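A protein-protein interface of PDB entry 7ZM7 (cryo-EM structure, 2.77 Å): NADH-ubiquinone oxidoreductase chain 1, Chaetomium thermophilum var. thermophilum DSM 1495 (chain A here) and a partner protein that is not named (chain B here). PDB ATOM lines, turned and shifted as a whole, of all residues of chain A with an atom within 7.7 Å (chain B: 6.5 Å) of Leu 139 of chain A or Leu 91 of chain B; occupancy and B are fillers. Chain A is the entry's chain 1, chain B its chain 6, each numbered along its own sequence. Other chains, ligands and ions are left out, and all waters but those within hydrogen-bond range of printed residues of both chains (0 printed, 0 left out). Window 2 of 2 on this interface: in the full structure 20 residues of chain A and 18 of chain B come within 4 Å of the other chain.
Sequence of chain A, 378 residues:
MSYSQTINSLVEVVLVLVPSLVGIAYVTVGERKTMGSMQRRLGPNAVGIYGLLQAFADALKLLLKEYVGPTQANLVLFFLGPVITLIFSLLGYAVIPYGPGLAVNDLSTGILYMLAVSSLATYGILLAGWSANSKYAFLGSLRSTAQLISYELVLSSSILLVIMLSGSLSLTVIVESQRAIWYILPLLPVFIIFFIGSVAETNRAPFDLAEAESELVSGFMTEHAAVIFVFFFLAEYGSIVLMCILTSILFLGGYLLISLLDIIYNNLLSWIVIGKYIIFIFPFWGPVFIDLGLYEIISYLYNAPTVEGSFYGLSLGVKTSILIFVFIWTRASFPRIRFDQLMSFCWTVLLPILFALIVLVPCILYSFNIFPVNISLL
Printed residues of chain B within 4 Å of Leu 139 of chain A: Leu 91 (3.9 Å).
Leu 91 of chain B touches just these residues of chain A: Leu 139 (3.9 Å) and Leu 142 (3.6 Å).
Of the printed residues of chain B, Leu 142 of chain A touches Phe 87, Met 90 and Leu 91.
Printed residues of chain B within 4 Å of Thr 145 of chain A: Phe 87.
The nearest residue of chain B that does not touch Leu 139 of chain A is Met 90 of chain B (6.0 Å).
Trp 130 of chain A touches Met 90 of chain B.
Met 90 of chain B touches Phe 138 of chain A (O to CZ, 3.0 Å).
Leu 139 of chain A touches Leu 91 of chain B (CD2 to CD2, 3.9 Å).
CD1 of Phe 87 of chain B touches CD2 of Leu 142 of chain A (3.9 Å).
Met 90 of chain B touches Leu 142 of chain A.
Leu 142 of chain A touches Leu 91 of chain B.
Thr 145 of chain A touches Phe 87 of chain B (CG2 to CZ, 3.9 Å).
Of the 17 printed residues of chain A, 5 touch a printed residue of chain B.
Hydrophobic or aromatic side chains of chain A within 4 Å of the printed part of chain B: Trp 130, Phe 138, Leu 139 and Leu 142.
Of the 9 printed residues of chain B, 3 touch a printed residue of chain A.
Printed residues of chain B that touch a printed residue of chain A: Phe 87, Met 90 and Leu 91.
Hydrophobic or aromatic side chains of chain B that line the printed part of chain A: Phe 87, Met 90 and Leu 91.
Among the printed residues, 7 pairs touch across the chains.
The backbone carbonyl oxygen (O) of Phe 138 of chain A is in hydrogen-bond range of the side-chain hydroxyl (OG) of Ser 141 of chain A.
The side-chain hydroxyl (OG1) of Thr 145 of chain A sits at hydrogen-bond distance from the backbone carbonyl oxygen (O) of Ser 141 of chain A (2.9 Å).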
ATOM      1  N   GLY A 129      37.477 -18.346  26.238  1.00  0.00           N
ATOM      2  CA  GLY A 129      37.185 -19.582  25.538  1.00  0.00           C
ATOM      3  C   GLY A 129      36.342 -19.396  24.298  1.00  0.00           C
ATOM      4  O   GLY A 129      36.201 -20.336  23.513  1.00  0.00           O
ATOM      5  N   TRP A 130      35.766 -18.211  24.116  1.00  0.00           N
ATOM      6  CA  TRP A 130      35.006 -17.918  22.909  1.00  0.00           C
ATOM      7  C   TRP A 130      35.920 -17.650  21.723  1.00  0.00           C
ATOM      8  O   TRP A 130      35.482 -17.742  20.571  1.00  0.00           O
ATOM      9  CB  TRP A 130      34.087 -16.725  23.169  1.00  0.00           C
ATOM     10  CG  TRP A 130      33.422 -16.156  21.973  1.00  0.00           C
ATOM     11  CD1 TRP A 130      33.872 -15.130  21.198  1.00  0.00           C
ATOM     12  CD2 TRP A 130      32.168 -16.555  21.422  1.00  0.00           C
ATOM     13  NE1 TRP A 130      32.979 -14.872  20.189  1.00  0.00           N
ATOM     14  CE2 TRP A 130      31.924 -15.736  20.306  1.00  0.00           C
ATOM     15  CE3 TRP A 130      31.229 -17.529  21.760  1.00  0.00           C
ATOM     16  CZ2 TRP A 130      30.780 -15.864  19.530  1.00  0.00           C
ATOM     17  CZ3 TRP A 130      30.107 -17.655  20.988  1.00  0.00           C
ATOM     18  CH2 TRP A 130      29.885 -16.829  19.890  1.00  0.00           C
ATOM     19  N   SER A 134      37.246 -24.470  17.977  1.00  0.00           N
ATOM     20  CA  SER A 134      37.178 -25.925  17.915  1.00  0.00           C
ATOM     21  C   SER A 134      35.954 -26.381  18.693  1.00  0.00           C
ATOM     22  O   SER A 134      35.846 -26.105  19.889  1.00  0.00           O
ATOM     23  CB  SER A 134      38.449 -26.550  18.472  1.00  0.00           C
ATOM     24  OG  SER A 134      39.533 -26.322  17.589  1.00  0.00           O
ATOM     25  N   LYS A 135      35.040 -27.092  18.025  1.00  0.00           N
ATOM     26  CA  LYS A 135      33.703 -27.290  18.576  1.00  0.00           C
ATOM     27  C   LYS A 135      33.745 -27.853  19.985  1.00  0.00           C
ATOM     28  O   LYS A 135      33.069 -27.338  20.883  1.00  0.00           O
ATOM     29  CB  LYS A 135      32.888 -28.212  17.670  1.00  0.00           C
ATOM     30  CG  LYS A 135      31.736 -28.906  18.378  1.00  0.00           C
ATOM     31  CD  LYS A 135      30.649 -27.939  18.795  1.00  0.00           C
ATOM     32  CE  LYS A 135      29.435 -28.678  19.340  1.00  0.00           C
ATOM     33  NZ  LYS A 135      28.834 -29.613  18.351  1.00  0.00           N
ATOM     34  N   TYR A 136      34.529 -28.902  20.202  1.00  0.00           N
ATOM     35  CA  TYR A 136      34.544 -29.524  21.515  1.00  0.00           C
ATOM     36  C   TYR A 136      35.165 -28.624  22.578  1.00  0.00           C
ATOM     37  O   TYR A 136      34.767 -28.693  23.742  1.00  0.00           O
ATOM     38  CB  TYR A 136      35.271 -30.866  21.462  1.00  0.00           C
ATOM     39  CG  TYR A 136      35.063 -31.655  22.722  1.00  0.00           C
ATOM     40  CD1 TYR A 136      33.962 -32.477  22.870  1.00  0.00           C
ATOM     41  CD2 TYR A 136      35.949 -31.546  23.782  1.00  0.00           C
ATOM     42  CE1 TYR A 136      33.753 -33.180  24.037  1.00  0.00           C
ATOM     43  CE2 TYR A 136      35.753 -32.229  24.941  1.00  0.00           C
ATOM     44  CZ  TYR A 136      34.656 -33.047  25.074  1.00  0.00           C
ATOM     45  OH  TYR A 136      34.477 -33.741  26.242  1.00  0.00           O
ATOM     46  N   ALA A 137      36.135 -27.790  22.208  1.00  0.00           N
ATOM     47  CA  ALA A 137      36.774 -26.915  23.184  1.00  0.00           C
ATOM     48  C   ALA A 137      35.846 -25.796  23.629  1.00  0.00           C
ATOM     49  O   ALA A 137      35.882 -25.380  24.789  1.00  0.00           O
ATOM     50  CB  ALA A 137      38.060 -26.332  22.611  1.00  0.00           C
ATOM     51  N   PHE A 138      35.030 -25.271  22.721  1.00  0.00           N
ATOM     52  CA  PHE A 138      34.090 -24.226  23.106  1.00  0.00           C
ATOM     53  C   PHE A 138      33.111 -24.731  24.155  1.00  0.00           C
ATOM     54  O   PHE A 138      32.773 -24.011  25.095  1.00  0.00           O
ATOM     55  CB  PHE A 138      33.340 -23.708  21.883  1.00  0.00           C
ATOM     56  CG  PHE A 138      32.067 -23.007  22.213  1.00  0.00           C
ATOM     57  CD1 PHE A 138      32.088 -21.766  22.811  1.00  0.00           C
ATOM     58  CD2 PHE A 138      30.843 -23.595  21.932  1.00  0.00           C
ATOM     59  CE1 PHE A 138      30.926 -21.114  23.121  1.00  0.00           C
ATOM     60  CE2 PHE A 138      29.664 -22.953  22.243  1.00  0.00           C
ATOM     61  CZ  PHE A 138      29.704 -21.712  22.840  1.00  0.00           C
ATOM     62  N   LEU A 139      32.629 -25.957  24.003  1.00  0.00           N
ATOM     63  CA  LEU A 139      31.757 -26.511  25.021  1.00  0.00           C
ATOM     64  C   LEU A 139      32.504 -26.739  26.323  1.00  0.00           C
ATOM     65  O   LEU A 139      31.882 -26.804  27.385  1.00  0.00           O
ATOM     66  CB  LEU A 139      31.129 -27.805  24.529  1.00  0.00           C
ATOM     67  CG  LEU A 139      30.475 -27.807  23.152  1.00  0.00           C
ATOM     68  CD1 LEU A 139      29.894 -29.166  22.880  1.00  0.00           C
ATOM     69  CD2 LEU A 139      29.412 -26.755  23.066  1.00  0.00           C
ATOM     70  N   GLY A 140      33.831 -26.841  26.270  1.00  0.00           N
ATOM     71  CA  GLY A 140      34.609 -26.953  27.487  1.00  0.00           C
ATOM     72  C   GLY A 140      34.758 -25.645  28.236  1.00  0.00           C
ATOM     73  O   GLY A 140      35.089 -25.639  29.423  1.00  0.00           O
ATOM     74  N   SER A 141      34.519 -24.532  27.545  1.00  0.00           N
ATOM     75  CA  SER A 141      34.559 -23.208  28.217  1.00  0.00           C
ATOM     76  C   SER A 141      33.204 -22.988  28.889  1.00  0.00           C
ATOM     77  O   SER A 141      33.165 -22.296  29.919  1.00  0.00           O
ATOM     78  CB  SER A 141      34.895 -22.107  27.247  1.00  0.00           C
ATOM     79  OG  SER A 141      33.795 -21.807  26.402  1.00  0.00           O
ATOM     80  N   LEU A 142      32.134 -23.511  28.287  1.00  0.00           N
ATOM     81  CA  LEU A 142      30.788 -23.432  28.902  1.00  0.00           C
ATOM     82  C   LEU A 142      30.772 -24.300  30.156  1.00  0.00           C
ATOM     83  O   LEU A 142      30.107 -23.912  31.127  1.00  0.00           O
ATOM     84  CB  LEU A 142      29.770 -23.962  27.894  1.00  0.00           C
ATOM     85  CG  LEU A 142      29.638 -23.173  26.595  1.00  0.00           C
ATOM     86  CD1 LEU A 142      28.560 -23.785  25.722  1.00  0.00           C
ATOM     87  CD2 LEU A 142      29.321 -21.716  26.880  1.00  0.00           C
ATOM     88  N   ARG A 143      31.435 -25.459  30.096  1.00  0.00           N
ATOM     89  CA  ARG A 143      31.453 -26.405  31.234  1.00  0.00           C
ATOM     90  C   ARG A 143      32.283 -25.796  32.362  1.00  0.00           C
ATOM     91  O   ARG A 143      31.932 -25.995  33.529  1.00  0.00           O
ATOM     92  CB  ARG A 143      31.965 -27.773  30.764  1.00  0.00           C
ATOM     93  CG  ARG A 143      30.861 -28.731  30.347  1.00  0.00           C
ATOM     94  CD  ARG A 143      31.316 -29.916  29.518  1.00  0.00           C
ATOM     95  NE  ARG A 143      32.425 -30.668  30.088  1.00  0.00           N
ATOM     96  CZ  ARG A 143      33.624 -30.771  29.531  1.00  0.00           C
ATOM     97  NH1 ARG A 143      33.872 -30.173  28.380  1.00  0.00           N
ATOM     98  NH2 ARG A 143      34.570 -31.480  30.123  1.00  0.00           N
ATOM     99  N   SER A 144      33.336 -25.064  32.025  1.00  0.00           N
ATOM    100  CA  SER A 144      34.104 -24.386  33.092  1.00  0.00           C
ATOM    101  C   SER A 144      33.256 -23.276  33.712  1.00  0.00           C
ATOM    102  O   SER A 144      33.345 -23.082  34.931  1.00  0.00           O
ATOM    103  CB  SER A 144      35.456 -23.932  32.621  1.00  0.00           C
ATOM    104  OG  SER A 144      35.355 -23.220  31.406  1.00  0.00           O
ATOM    105  N   THR A 145      32.473 -22.575  32.900  1.00  0.00           N
ATOM    106  CA  THR A 145      31.561 -21.523  33.423  1.00  0.00           C
ATOM    107  C   THR A 145      30.512 -22.176  34.326  1.00  0.00           C
ATOM    108  O   THR A 145      30.237 -21.632  35.402  1.00  0.00           O
ATOM    109  CB  THR A 145      31.006 -20.645  32.292  1.00  0.00           C
ATOM    110  OG1 THR A 145      32.118 -20.126  31.564  1.00  0.00           O
ATOM    111  CG2 THR A 145      30.168 -19.490  32.791  1.00  0.00           C
ATOM    112  N   ALA A 146      29.993 -23.324  33.918  1.00  0.00           N
ATOM    113  CA  ALA A 146      28.997 -24.059  34.719  1.00  0.00           C
ATOM    114  C   ALA A 146      29.600 -24.472  36.064  1.00  0.00           C
ATOM    115  O   ALA A 146      28.870 -24.440  37.067  1.00  0.00           O
ATOM    116  CB  ALA A 146      28.521 -25.234  33.921  1.00  0.00           C
ATOM    117  N   ALA A 210      37.617 -29.776  32.778  1.00  0.00           N
ATOM    118  CA  ALA A 210      36.896 -29.196  31.652  1.00  0.00           C
ATOM    119  C   ALA A 210      37.818 -28.348  30.790  1.00  0.00           C
ATOM    120  O   ALA A 210      37.877 -28.532  29.571  1.00  0.00           O
ATOM    121  CB  ALA A 210      35.701 -28.380  32.135  1.00  0.00           C
ATOM    122  N   PHE A 339      33.884 -33.756  34.870  1.00  0.00           N
ATOM    123  CA  PHE A 339      32.942 -32.623  35.063  1.00  0.00           C
ATOM    124  C   PHE A 339      31.612 -33.082  35.673  1.00  0.00           C
ATOM    125  O   PHE A 339      31.142 -32.416  36.591  1.00  0.00           O
ATOM    126  CB  PHE A 339      32.752 -31.825  33.768  1.00  0.00           C
ATOM    127  CG  PHE A 339      31.654 -30.796  33.813  1.00  0.00           C
ATOM    128  CD1 PHE A 339      31.881 -29.544  34.357  1.00  0.00           C
ATOM    129  CD2 PHE A 339      30.394 -31.084  33.316  1.00  0.00           C
ATOM    130  CE1 PHE A 339      30.863 -28.606  34.410  1.00  0.00           C
ATOM    131  CE2 PHE A 339      29.381 -30.142  33.366  1.00  0.00           C
ATOM    132  CZ  PHE A 339      29.620 -28.902  33.906  1.00  0.00           C
ATOM    133  N   LEU B  86      23.776 -15.796  27.764  1.00  0.00           N
ATOM    134  CA  LEU B  86      24.951 -16.130  26.970  1.00  0.00           C
ATOM    135  C   LEU B  86      25.003 -17.617  26.629  1.00  0.00           C
ATOM    136  O   LEU B  86      25.237 -17.969  25.473  1.00  0.00           O
ATOM    137  CB  LEU B  86      26.210 -15.677  27.698  1.00  0.00           C
ATOM    138  CG  LEU B  86      26.480 -14.177  27.569  1.00  0.00           C
ATOM    139  CD1 LEU B  86      27.481 -13.721  28.590  1.00  0.00           C
ATOM    140  CD2 LEU B  86      26.946 -13.833  26.184  1.00  0.00           C
ATOM    141  N   PHE B  87      24.775 -18.507  27.603  1.00  0.00           N
ATOM    142  CA  PHE B  87      24.663 -19.930  27.278  1.00  0.00           C
ATOM    143  C   PHE B  87      23.752 -20.179  26.087  1.00  0.00           C
ATOM    144  O   PHE B  87      24.186 -20.724  25.068  1.00  0.00           O
ATOM    145  CB  PHE B  87      24.162 -20.754  28.469  1.00  0.00           C
ATOM    146  CG  PHE B  87      25.151 -20.923  29.576  1.00  0.00           C
ATOM    147  CD1 PHE B  87      26.489 -20.642  29.384  1.00  0.00           C
ATOM    148  CD2 PHE B  87      24.755 -21.461  30.784  1.00  0.00           C
ATOM    149  CE1 PHE B  87      27.405 -20.843  30.395  1.00  0.00           C
ATOM    150  CE2 PHE B  87      25.676 -21.673  31.794  1.00  0.00           C
ATOM    151  CZ  PHE B  87      27.000 -21.357  31.601  1.00  0.00           C
ATOM    152  N   ILE B  88      22.488 -19.781  26.190  1.00  0.00           N
ATOM    153  CA  ILE B  88      21.549 -20.100  25.127  1.00  0.00           C
ATOM    154  C   ILE B  88      21.989 -19.467  23.813  1.00  0.00           C
ATOM    155  O   ILE B  88      21.904 -20.090  22.754  1.00  0.00           O
ATOM    156  CB  ILE B  88      20.124 -19.678  25.525  1.00  0.00           C
ATOM    157  CG1 ILE B  88      19.710 -20.416  26.787  1.00  0.00           C
ATOM    158  CG2 ILE B  88      19.148 -19.962  24.412  1.00  0.00           C
ATOM    159  CD1 ILE B  88      19.717 -21.900  26.623  1.00  0.00           C
ATOM    160  N   LEU B  89      22.482 -18.240  23.858  1.00  0.00           N
ATOM    161  CA  LEU B  89      22.795 -17.564  22.613  1.00  0.00           C
ATOM    162  C   LEU B  89      24.066 -18.087  21.962  1.00  0.00           C
ATOM    163  O   LEU B  89      24.269 -17.868  20.768  1.00  0.00           O
ATOM    164  CB  LEU B  89      22.907 -16.072  22.857  1.00  0.00           C
ATOM    165  CG  LEU B  89      21.650 -15.217  22.904  1.00  0.00           C
ATOM    166  CD1 LEU B  89      22.063 -13.778  22.824  1.00  0.00           C
ATOM    167  CD2 LEU B  89      20.716 -15.556  21.793  1.00  0.00           C
ATOM    168  N   MET B  90      24.922 -18.770  22.707  1.00  0.00           N
ATOM    169  CA  MET B  90      26.137 -19.344  22.154  1.00  0.00           C
ATOM    170  C   MET B  90      25.985 -20.819  21.826  1.00  0.00           C
ATOM    171  O   MET B  90      26.984 -21.480  21.559  1.00  0.00           O
ATOM    172  CB  MET B  90      27.305 -19.121  23.116  1.00  0.00           C
ATOM    173  CG  MET B  90      27.593 -17.646  23.312  1.00  0.00           C
ATOM    174  SD  MET B  90      28.501 -17.146  24.784  1.00  0.00           S
ATOM    175  CE  MET B  90      29.533 -18.544  25.074  1.00  0.00           C
ATOM    176  N   LEU B  91      24.774 -21.342  21.835  1.00  0.00           N
ATOM    177  CA  LEU B  91      24.484 -22.727  21.502  1.00  0.00           C
ATOM    178  C   LEU B  91      23.394 -22.862  20.460  1.00  0.00           C
ATOM    179  O   LEU B  91      23.461 -23.747  19.613  1.00  0.00           O
ATOM    180  CB  LEU B  91      24.066 -23.486  22.749  1.00  0.00           C
ATOM    181  CG  LEU B  91      25.118 -23.691  23.814  1.00  0.00           C
ATOM    182  CD1 LEU B  91      24.427 -24.096  25.096  1.00  0.00           C
ATOM    183  CD2 LEU B  91      26.085 -24.751  23.350  1.00  0.00           C
ATOM    184  N   ILE B  92      22.371 -22.014  20.519  1.00  0.00           N
ATOM    185  CA  ILE B  92      21.429 -21.914  19.421  1.00  0.00           C
ATOM    186  C   ILE B  92      22.166 -21.484  18.166  1.00  0.00           C
ATOM    187  O   ILE B  92      23.038 -20.607  18.198  1.00  0.00           O
ATOM    188  CB  ILE B  92      20.305 -20.932  19.778  1.00  0.00           C
ATOM    189  CG1 ILE B  92      19.348 -21.574  20.777  1.00  0.00           C
ATOM    190  CG2 ILE B  92      19.593 -20.459  18.549  1.00  0.00           C
ATOM    191  CD1 ILE B  92      18.112 -20.754  21.030  1.00  0.00           C
ATOM    192  N   ASN B  93      21.855 -22.133  17.057  1.00  0.00           N
ATOM    193  CA  ASN B  93      22.388 -21.693  15.781  1.00  0.00           C
ATOM    194  C   ASN B  93      21.692 -20.407  15.376  1.00  0.00           C
ATOM    195  O   ASN B  93      20.463 -20.348  15.328  1.00  0.00           O
ATOM    196  CB  ASN B  93      22.208 -22.783  14.733  1.00  0.00           C
ATOM    197  CG  ASN B  93      23.129 -23.954  14.960  1.00  0.00           C
ATOM    198  OD1 ASN B  93      22.693 -25.042  15.328  1.00  0.00           O
ATOM    199  ND2 ASN B  93      24.421 -23.738  14.745  1.00  0.00           N
ATOM    200  N   ILE B  94      22.467 -19.367  15.116  1.00  0.00           N
ATOM    201  CA  ILE B  94      21.933 -18.068  14.745  1.00  0.00           C
ATOM    202  C   ILE B  94      22.595 -17.637  13.451  1.00  0.00           C
ATOM    203  O   ILE B  94      23.807 -17.397  13.414  1.00  0.00           O
ATOM    204  CB  ILE B  94      22.157 -17.020  15.843  1.00  0.00           C
ATOM    205  CG1 ILE B  94      21.430 -17.414  17.125  1.00  0.00           C
ATOM    206  CG2 ILE B  94      21.694 -15.661  15.368  1.00  0.00           C
ATOM    207  CD1 ILE B  94      22.213 -17.146  18.375  1.00  0.00           C
